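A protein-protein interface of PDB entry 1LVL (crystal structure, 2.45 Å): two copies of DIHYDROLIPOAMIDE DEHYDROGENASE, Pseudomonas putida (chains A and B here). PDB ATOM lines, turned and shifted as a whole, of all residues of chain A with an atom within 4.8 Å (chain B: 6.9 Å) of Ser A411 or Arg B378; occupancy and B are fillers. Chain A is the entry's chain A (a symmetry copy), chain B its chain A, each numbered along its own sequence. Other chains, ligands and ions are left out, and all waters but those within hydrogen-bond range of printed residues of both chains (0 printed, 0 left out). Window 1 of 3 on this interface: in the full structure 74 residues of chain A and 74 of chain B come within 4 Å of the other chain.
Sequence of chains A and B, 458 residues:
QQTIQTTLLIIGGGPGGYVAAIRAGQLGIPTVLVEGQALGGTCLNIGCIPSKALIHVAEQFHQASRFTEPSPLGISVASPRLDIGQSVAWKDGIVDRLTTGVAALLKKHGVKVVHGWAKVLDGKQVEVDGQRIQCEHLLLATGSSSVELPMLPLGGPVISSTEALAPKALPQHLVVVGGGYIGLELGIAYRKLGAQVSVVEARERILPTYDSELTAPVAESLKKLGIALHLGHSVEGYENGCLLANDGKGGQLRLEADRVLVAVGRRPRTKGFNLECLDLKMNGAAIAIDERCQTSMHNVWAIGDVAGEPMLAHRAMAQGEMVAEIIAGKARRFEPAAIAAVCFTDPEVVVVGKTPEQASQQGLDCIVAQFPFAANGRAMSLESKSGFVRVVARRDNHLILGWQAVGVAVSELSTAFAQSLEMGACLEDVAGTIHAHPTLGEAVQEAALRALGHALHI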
ATOM      1  N   VAL A 342      30.915  -6.887   8.522  1.00  0.00           N
ATOM      2  CA  VAL A 342      29.585  -6.347   8.507  1.00  0.00           C
ATOM      3  C   VAL A 342      29.654  -4.844   8.215  1.00  0.00           C
ATOM      4  O   VAL A 342      30.594  -4.247   8.728  1.00  0.00           O
ATOM      5  CB  VAL A 342      28.895  -6.665   9.895  1.00  0.00           C
ATOM      6  CG1 VAL A 342      27.482  -6.169  10.010  1.00  0.00           C
ATOM      7  CG2 VAL A 342      28.670  -8.133   9.984  1.00  0.00           C
ATOM      8  N   PHE A 344      27.247  -1.509   8.671  1.00  0.00           N
ATOM      9  CA  PHE A 344      26.008  -0.982   9.146  1.00  0.00           C
ATOM     10  C   PHE A 344      25.517   0.176   8.273  1.00  0.00           C
ATOM     11  O   PHE A 344      25.167   1.276   8.744  1.00  0.00           O
ATOM     12  CB  PHE A 344      26.176  -0.582  10.616  1.00  0.00           C
ATOM     13  CG  PHE A 344      26.366  -1.854  11.459  1.00  0.00           C
ATOM     14  CD1 PHE A 344      27.592  -2.476  11.561  1.00  0.00           C
ATOM     15  CD2 PHE A 344      25.288  -2.429  12.100  1.00  0.00           C
ATOM     16  CE1 PHE A 344      27.744  -3.649  12.276  1.00  0.00           C
ATOM     17  CE2 PHE A 344      25.448  -3.598  12.805  1.00  0.00           C
ATOM     18  CZ  PHE A 344      26.664  -4.211  12.898  1.00  0.00           C
ATOM     19  N   GLU A 348      22.176  -3.239   5.296  1.00  0.00           N
ATOM     20  CA  GLU A 348      23.360  -3.756   5.856  1.00  0.00           C
ATOM     21  C   GLU A 348      23.792  -4.823   4.954  1.00  0.00           C
ATOM     22  O   GLU A 348      22.969  -5.595   4.506  1.00  0.00           O
ATOM     23  CB  GLU A 348      23.084  -4.361   7.189  1.00  0.00           C
ATOM     24  CG  GLU A 348      22.437  -3.330   8.048  1.00  0.00           C
ATOM     25  CD  GLU A 348      22.037  -3.808   9.420  1.00  0.00           C
ATOM     26  OE1 GLU A 348      22.190  -4.993   9.742  1.00  0.00           O
ATOM     27  OE2 GLU A 348      21.557  -2.959  10.165  1.00  0.00           O
ATOM     28  N   VAL A 350      26.657  -8.006   4.785  1.00  0.00           N
ATOM     29  CA  VAL A 350      27.260  -8.969   5.648  1.00  0.00           C
ATOM     30  C   VAL A 350      27.908  -9.844   4.619  1.00  0.00           C
ATOM     31  O   VAL A 350      27.199 -10.232   3.697  1.00  0.00           O
ATOM     32  CB  VAL A 350      26.237  -9.896   6.418  1.00  0.00           C
ATOM     33  CG1 VAL A 350      26.989 -10.979   7.177  1.00  0.00           C
ATOM     34  CG2 VAL A 350      25.409  -9.124   7.412  1.00  0.00           C
ATOM     35  N   ALA A 409      18.184  -5.140   9.178  1.00  0.00           N
ATOM     36  CA  ALA A 409      18.446  -6.076  10.280  1.00  0.00           C
ATOM     37  C   ALA A 409      19.092  -7.423  10.054  1.00  0.00           C
ATOM     38  O   ALA A 409      19.067  -8.400  10.838  1.00  0.00           O
ATOM     39  CB  ALA A 409      17.138  -6.290  11.028  1.00  0.00           C
ATOM     40  N   VAL A 410      19.897  -7.372   9.002  1.00  0.00           N
ATOM     41  CA  VAL A 410      20.612  -8.576   8.625  1.00  0.00           C
ATOM     42  C   VAL A 410      21.873  -8.865   9.428  1.00  0.00           C
ATOM     43  O   VAL A 410      22.366 -10.008   9.436  1.00  0.00           O
ATOM     44  CB  VAL A 410      20.817  -8.362   7.116  1.00  0.00           C
ATOM     45  CG1 VAL A 410      22.233  -8.077   6.600  1.00  0.00           C
ATOM     46  CG2 VAL A 410      20.301  -9.646   6.585  1.00  0.00           C
ATOM     47  N   SER A 411      22.425  -7.858  10.132  1.00  0.00           N
ATOM     48  CA  SER A 411      23.733  -8.014  10.784  1.00  0.00           C
ATOM     49  C   SER A 411      23.868  -9.224  11.638  1.00  0.00           C
ATOM     50  O   SER A 411      24.906  -9.890  11.559  1.00  0.00           O
ATOM     51  CB  SER A 411      24.056  -6.815  11.646  1.00  0.00           C
ATOM     52  OG  SER A 411      22.925  -6.225  12.284  1.00  0.00           O
ATOM     53  N   GLU A 412      22.760  -9.597  12.329  1.00  0.00           N
ATOM     54  CA  GLU A 412      22.764 -10.752  13.228  1.00  0.00           C
ATOM     55  C   GLU A 412      22.721 -12.111  12.587  1.00  0.00           C
ATOM     56  O   GLU A 412      22.895 -13.138  13.249  1.00  0.00           O
ATOM     57  CB  GLU A 412      21.615 -10.627  14.246  1.00  0.00           C
ATOM     58  CG  GLU A 412      21.615  -9.389  15.230  1.00  0.00           C
ATOM     59  CD  GLU A 412      22.909  -8.984  15.964  1.00  0.00           C
ATOM     60  OE1 GLU A 412      23.708  -9.847  16.296  1.00  0.00           O
ATOM     61  OE2 GLU A 412      23.131  -7.788  16.191  1.00  0.00           O
ATOM     62  N   LEU A 413      22.598 -12.169  11.276  1.00  0.00           N
ATOM     63  CA  LEU A 413      22.710 -13.460  10.603  1.00  0.00           C
ATOM     64  C   LEU A 413      24.143 -13.896  10.508  1.00  0.00           C
ATOM     65  O   LEU A 413      24.388 -15.120  10.344  1.00  0.00           O
ATOM     66  CB  LEU A 413      22.127 -13.376   9.219  1.00  0.00           C
ATOM     67  CG  LEU A 413      20.674 -13.013   9.174  1.00  0.00           C
ATOM     68  CD1 LEU A 413      20.175 -13.178   7.747  1.00  0.00           C
ATOM     69  CD2 LEU A 413      19.897 -13.920  10.117  1.00  0.00           C
ATOM     70  N   SER A 414      25.093 -12.916  10.654  1.00  0.00           N
ATOM     71  CA  SER A 414      26.545 -13.241  10.644  1.00  0.00           C
ATOM     72  C   SER A 414      26.987 -14.302  11.598  1.00  0.00           C
ATOM     73  O   SER A 414      27.860 -15.092  11.230  1.00  0.00           O
ATOM     74  CB  SER A 414      27.431 -12.023  10.940  1.00  0.00           C
ATOM     75  OG  SER A 414      26.930 -11.147  11.935  1.00  0.00           O
ATOM     76  N   PHE B 373      23.653  -8.663  28.401  1.00  0.00           N
ATOM     77  CA  PHE B 373      23.849  -7.609  27.422  1.00  0.00           C
ATOM     78  C   PHE B 373      24.354  -6.283  27.993  1.00  0.00           C
ATOM     79  O   PHE B 373      24.716  -5.387  27.224  1.00  0.00           O
ATOM     80  CB  PHE B 373      22.533  -7.407  26.637  1.00  0.00           C
ATOM     81  CG  PHE B 373      22.296  -8.587  25.700  1.00  0.00           C
ATOM     82  CD1 PHE B 373      23.305  -9.082  24.910  1.00  0.00           C
ATOM     83  CD2 PHE B 373      21.076  -9.206  25.658  1.00  0.00           C
ATOM     84  CE1 PHE B 373      23.108 -10.180  24.094  1.00  0.00           C
ATOM     85  CE2 PHE B 373      20.897 -10.299  24.841  1.00  0.00           C
ATOM     86  CZ  PHE B 373      21.898 -10.806  24.051  1.00  0.00           C
ATOM     87  N   ASN B 376      27.843  -5.663  26.788  1.00  0.00           N
ATOM     88  CA  ASN B 376      27.818  -5.889  25.336  1.00  0.00           C
ATOM     89  C   ASN B 376      27.635  -4.529  24.701  1.00  0.00           C
ATOM     90  O   ASN B 376      26.670  -3.816  24.990  1.00  0.00           O
ATOM     91  CB  ASN B 376      26.626  -6.824  24.878  1.00  0.00           C
ATOM     92  CG  ASN B 376      26.491  -7.050  23.357  1.00  0.00           C
ATOM     93  OD1 ASN B 376      27.029  -7.944  22.722  1.00  0.00           O
ATOM     94  ND2 ASN B 376      25.838  -6.214  22.608  1.00  0.00           N
ATOM     95  N   GLY B 377      28.565  -4.181  23.805  1.00  0.00           N
ATOM     96  CA  GLY B 377      28.542  -2.908  23.123  1.00  0.00           C
ATOM     97  C   GLY B 377      27.382  -2.695  22.177  1.00  0.00           C
ATOM     98  O   GLY B 377      26.738  -1.625  22.207  1.00  0.00           O
ATOM     99  N   ARG B 378      27.112  -3.710  21.339  1.00  0.00           N
ATOM    100  CA  ARG B 378      25.987  -3.655  20.430  1.00  0.00           C
ATOM    101  C   ARG B 378      24.746  -3.348  21.259  1.00  0.00           C
ATOM    102  O   ARG B 378      24.204  -2.268  21.098  1.00  0.00           O
ATOM    103  CB  ARG B 378      25.869  -4.984  19.676  1.00  0.00           C
ATOM    104  CG  ARG B 378      24.792  -4.894  18.614  1.00  0.00           C
ATOM    105  CD  ARG B 378      25.104  -3.703  17.742  1.00  0.00           C
ATOM    106  NE  ARG B 378      24.073  -3.030  16.973  1.00  0.00           N
ATOM    107  CZ  ARG B 378      23.349  -3.654  16.042  1.00  0.00           C
ATOM    108  NH1 ARG B 378      23.451  -4.990  15.728  1.00  0.00           N
ATOM    109  NH2 ARG B 378      22.596  -2.808  15.325  1.00  0.00           N
ATOM    110  N   ALA B 379      24.274  -4.188  22.164  1.00  0.00           N
ATOM    111  CA  ALA B 379      23.218  -3.865  23.118  1.00  0.00           C
ATOM    112  C   ALA B 379      23.175  -2.436  23.594  1.00  0.00           C
ATOM    113  O   ALA B 379      22.141  -1.805  23.495  1.00  0.00           O
ATOM    114  CB  ALA B 379      23.353  -4.768  24.324  1.00  0.00           C
ATOM    115  N   MET B 380      24.278  -1.832  24.001  1.00  0.00           N
ATOM    116  CA  MET B 380      24.314  -0.423  24.376  1.00  0.00           C
ATOM    117  C   MET B 380      24.085   0.510  23.211  1.00  0.00           C
ATOM    118  O   MET B 380      23.414   1.535  23.412  1.00  0.00           O
ATOM    119  CB  MET B 380      25.648  -0.032  25.003  1.00  0.00           C
ATOM    120  CG  MET B 380      25.970  -0.782  26.273  1.00  0.00           C
ATOM    121  SD  MET B 380      27.529  -0.284  27.029  1.00  0.00           S
ATOM    122  CE  MET B 380      28.019  -1.963  27.279  1.00  0.00           C
ATOM    123  N   SER B 381      24.573   0.237  21.998  1.00  0.00           N
ATOM    124  CA  SER B 381      24.206   1.139  20.909  1.00  0.00           C
ATOM    125  C   SER B 381      22.711   1.217  20.725  1.00  0.00           C
ATOM    126  O   SER B 381      22.167   2.262  20.424  1.00  0.00           O
ATOM    127  CB  SER B 381      24.820   0.724  19.577  1.00  0.00           C
ATOM    128  OG  SER B 381      24.826  -0.618  19.074  1.00  0.00           O
ATOM    129  N   LEU B 382      22.040   0.116  21.039  1.00  0.00           N
ATOM    130  CA  LEU B 382      20.622  -0.133  20.861  1.00  0.00           C
ATOM    131  C   LEU B 382      19.686   0.210  22.000  1.00  0.00           C
ATOM    132  O   LEU B 382      18.511  -0.160  22.004  1.00  0.00           O
ATOM    133  CB  LEU B 382      20.551  -1.589  20.524  1.00  0.00           C
ATOM    134  CG  LEU B 382      20.225  -2.117  19.133  1.00  0.00           C
ATOM    135  CD1 LEU B 382      20.610  -1.106  18.055  1.00  0.00           C
ATOM    136  CD2 LEU B 382      20.873  -3.482  19.005  1.00  0.00           C
ATOM    137  N   GLU B 383      20.152   0.922  23.012  1.00  0.00           N
ATOM    138  CA  GLU B 383      19.439   1.206  24.258  1.00  0.00           C
ATOM    139  C   GLU B 383      19.022  -0.046  25.026  1.00  0.00           C
ATOM    140  O   GLU B 383      18.057  -0.127  25.767  1.00  0.00           O
ATOM    141  CB  GLU B 383      18.237   2.073  23.961  1.00  0.00           C
ATOM    142  CG  GLU B 383      18.733   3.428  23.535  1.00  0.00           C
ATOM    143  CD  GLU B 383      17.610   4.376  23.208  1.00  0.00           C
ATOM    144  OE1 GLU B 383      17.062   4.988  24.127  1.00  0.00           O
ATOM    145  OE2 GLU B 383      17.305   4.496  22.027  1.00  0.00           O
ATOM    146  N   SER B 384      19.851  -1.040  24.796  1.00  0.00           N
ATOM    147  CA  SER B 384      19.945  -2.313  25.448  1.00  0.00           C
ATOM    148  C   SER B 384      18.811  -3.280  25.582  1.00  0.00           C
ATOM    149  O   SER B 384      18.800  -4.304  24.899  1.00  0.00           O
ATOM    150  CB  SER B 384      20.555  -2.038  26.842  1.00  0.00           C
ATOM    151  OG  SER B 384      21.423  -3.027  27.381  1.00  0.00           O
ATOM    152  N   VAL B 408      16.470  -7.262  23.577  1.00  0.00           N
ATOM    153  CA  VAL B 408      16.116  -6.513  22.388  1.00  0.00           C
ATOM    154  C   VAL B 408      16.674  -7.263  21.135  1.00  0.00           C
ATOM    155  O   VAL B 408      17.626  -8.045  21.278  1.00  0.00           O
ATOM    156  CB  VAL B 408      16.717  -5.104  22.657  1.00  0.00           C
ATOM    157  CG1 VAL B 408      18.019  -4.897  21.872  1.00  0.00           C
ATOM    158  CG2 VAL B 408      15.656  -4.066  22.392  1.00  0.00           C
ATOM    159  N   ALA B 409      16.044  -7.210  19.927  1.00  0.00           N
ATOM    160  CA  ALA B 409      16.560  -7.803  18.686  1.00  0.00           C
ATOM    161  C   ALA B 409      17.275  -9.133  18.667  1.00  0.00           C
ATOM    162  O   ALA B 409      18.016  -9.565  17.755  1.00  0.00           O
ATOM    163  CB  ALA B 409      17.451  -6.769  18.013  1.00  0.00           C
ATOM    164  N   ALA B 436      31.604 -11.336  14.883  1.00  0.00           N
ATOM    165  CA  ALA B 436      31.813 -10.019  14.429  1.00  0.00           C
ATOM    166  C   ALA B 436      31.398  -8.963  15.381  1.00  0.00           C
ATOM    167  O   ALA B 436      30.349  -9.080  15.985  1.00  0.00           O
ATOM    168  CB  ALA B 436      31.069  -9.824  13.087  1.00  0.00           C
ATOM    169  N   HIS B 437      32.187  -7.875  15.430  1.00  0.00           N
ATOM    170  CA  HIS B 437      32.025  -6.760  16.368  1.00  0.00           C
ATOM    171  C   HIS B 437      31.494  -5.538  15.619  1.00  0.00           C
ATOM    172  O   HIS B 437      31.861  -5.284  14.475  1.00  0.00           O
ATOM    173  CB  HIS B 437      33.436  -6.468  17.071  1.00  0.00           C
ATOM    174  CG  HIS B 437      33.440  -5.420  18.191  1.00  0.00           C
ATOM    175  ND1 HIS B 437      33.205  -5.803  19.448  1.00  0.00           N
ATOM    176  CD2 HIS B 437      33.336  -4.046  18.079  1.00  0.00           C
ATOM    177  CE1 HIS B 437      32.933  -4.680  20.108  1.00  0.00           C
ATOM    178  NE2 HIS B 437      33.010  -3.626  19.301  1.00  0.00           N
ATOM    179  N   PRO B 438      30.622  -4.724  16.200  1.00  0.00           N
ATOM    180  CA  PRO B 438      29.909  -5.026  17.432  1.00  0.00           C
ATOM    181  C   PRO B 438      28.620  -5.795  17.172  1.00  0.00           C
ATOM    182  O   PRO B 438      27.654  -5.133  16.764  1.00  0.00           O
ATOM    183  CB  PRO B 438      29.686  -3.639  18.053  1.00  0.00           C
ATOM    184  CG  PRO B 438      29.481  -2.702  16.904  1.00  0.00           C
ATOM    185  CD  PRO B 438      30.372  -3.346  15.765  1.00  0.00           C
ATOM    186  N   THR B 439      28.469  -7.123  17.296  1.00  0.00           N
ATOM    187  CA  THR B 439      27.101  -7.624  17.201  1.00  0.00           C
ATOM    188  C   THR B 439      26.523  -8.253  18.508  1.00  0.00           C
ATOM    189  O   THR B 439      27.284  -8.762  19.347  1.00  0.00           O
ATOM    190  CB  THR B 439      27.065  -8.615  15.965  1.00  0.00           C
ATOM    191  OG1 THR B 439      27.828  -9.781  16.305  1.00  0.00           O
ATOM    192  CG2 THR B 439      27.522  -7.909  14.663  1.00  0.00           C
ATOM    193  N   LEU B 440      25.186  -8.245  18.772  1.00  0.00           N
ATOM    194  CA  LEU B 440      24.531  -9.017  19.872  1.00  0.00           C
ATOM    195  C   LEU B 440      24.997 -10.486  19.953  1.00  0.00           C
ATOM    196  O   LEU B 440      25.102 -11.088  20.995  1.00  0.00           O
ATOM    197  CB  LEU B 440      23.033  -9.012  19.677  1.00  0.00           C
ATOM    198  CG  LEU B 440      22.079  -8.039  20.294  1.00  0.00           C
ATOM    199  CD1 LEU B 440      22.730  -6.797  20.765  1.00  0.00           C
ATOM    200  CD2 LEU B 440      21.020  -7.784  19.287  1.00  0.00           C
ATOM    201  N   GLY B 441      25.516 -11.091  18.920  1.00  0.00           N
ATOM    202  CA  GLY B 441      25.923 -12.468  18.921  1.00  0.00           C
ATOM    203  C   GLY B 441      27.269 -12.680  19.442  1.00  0.00           C
ATOM    204  O   GLY B 441      27.754 -13.834  19.508  1.00  0.00           O
ATOM    205  N   GLU B 442      27.876 -11.565  19.823  1.00  0.00           N
ATOM    206  CA  GLU B 442      29.153 -11.688  20.499  1.00  0.00           C
ATOM    207  C   GLU B 442      28.840 -12.346  21.831  1.00  0.00           C
ATOM    208  O   GLU B 442      29.544 -13.296  22.198  1.00  0.00           O
ATOM    209  CB  GLU B 442      29.733 -10.358  20.724  1.00  0.00           C
ATOM    210  CG  GLU B 442      30.376  -9.867  19.450  1.00  0.00           C
ATOM    211  CD  GLU B 442      31.144  -8.578  19.666  1.00  0.00           C
ATOM    212  OE1 GLU B 442      30.504  -7.511  19.732  1.00  0.00           O
ATOM    213  OE2 GLU B 442      32.373  -8.686  19.755  1.00  0.00           O
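The side-chain carboxylate (OE2) of Glu A412 is in salt-bridge range of the guanidinium group (NH1) of Arg B378 (2.9 Å). The side-chain carboxylate of Glu A412 sits at hydrogen-bond distance from the backbone NH of Leu B440. The backbone NH of Gly B441 is in hydrogen-bond range of the side-chain carboxylate of Glu A412 (3.4 Å).
The side-chain amide nitrogen (ND2) of Asn B376 lies close to the backbone NH (N) of Arg B378 (3.1 Å). OD1 of Asn B376 lies close to O of Thr B439 (3.5 Å). OG of Ser B381 lies within hydrogen-bond range of O of Arg B378, at 2.7 Å. The backbone carbonyl oxygen (O) of Ala B436 lies within hydrogen-bond range of the side-chain hydroxyl (OG1) of Thr B439, 2.6 Å away. N of Thr B439 sits at hydrogen-bond distance from OE1 of Glu B442 (3.2 Å). The backbone NH of Ser A411 lies within hydrogen-bond range of the side-chain carboxylate of Glu A348 (2.9 Å).
Among the printed residues, pairs that only touch across the chains: Phe A344 with Arg B378 (3.8 Å), Ser A411 with Arg B378 (3.7 Å) and Glu A412 with Thr B439 (3.6 Å).
Ser A411 touches one residue of chain B. Arg B378 touches just these residues of chain A: Phe A344 (3.8 Å), Ser A411 (3.7 Å) and Glu A412 (2.9 Å). Of the printed residues of chain A, Thr B439 touches Glu A412 (3.6 Å). Of the printed residues of chain A, Leu B440 touches Glu A412 (3.3 Å). Of the printed residues of chain A, Gly B441 touches Glu A412 (3.4 Å). Of the printed residues of chain B, Glu A412 touches Arg B378, Thr B439, Leu B440 and Gly B441. Glu B383 touches none of the printed residues of chain A. Ser B381 touches none of the printed residues of chain A. The nearest printed residue of chain A that does not touch Leu B440 is Ser A411 (7.2 Å).
Of the 10 printed residues of chain A, 3 touch a printed residue of chain B. Hydrophobic or aromatic side chains of chain B that line the printed part of chain A: Leu B440. Along chain B the printed residues that touch a printed residue of chain A span positions 378 to 441. Among the printed residues, 6 pairs touch across the chains. Among the printed residues, Asp or Glu carboxylates within 4 Å of a Lys or Arg side-chain nitrogen of the other chain: Glu A412 with Arg B378.
Position printed for both chains: 409.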
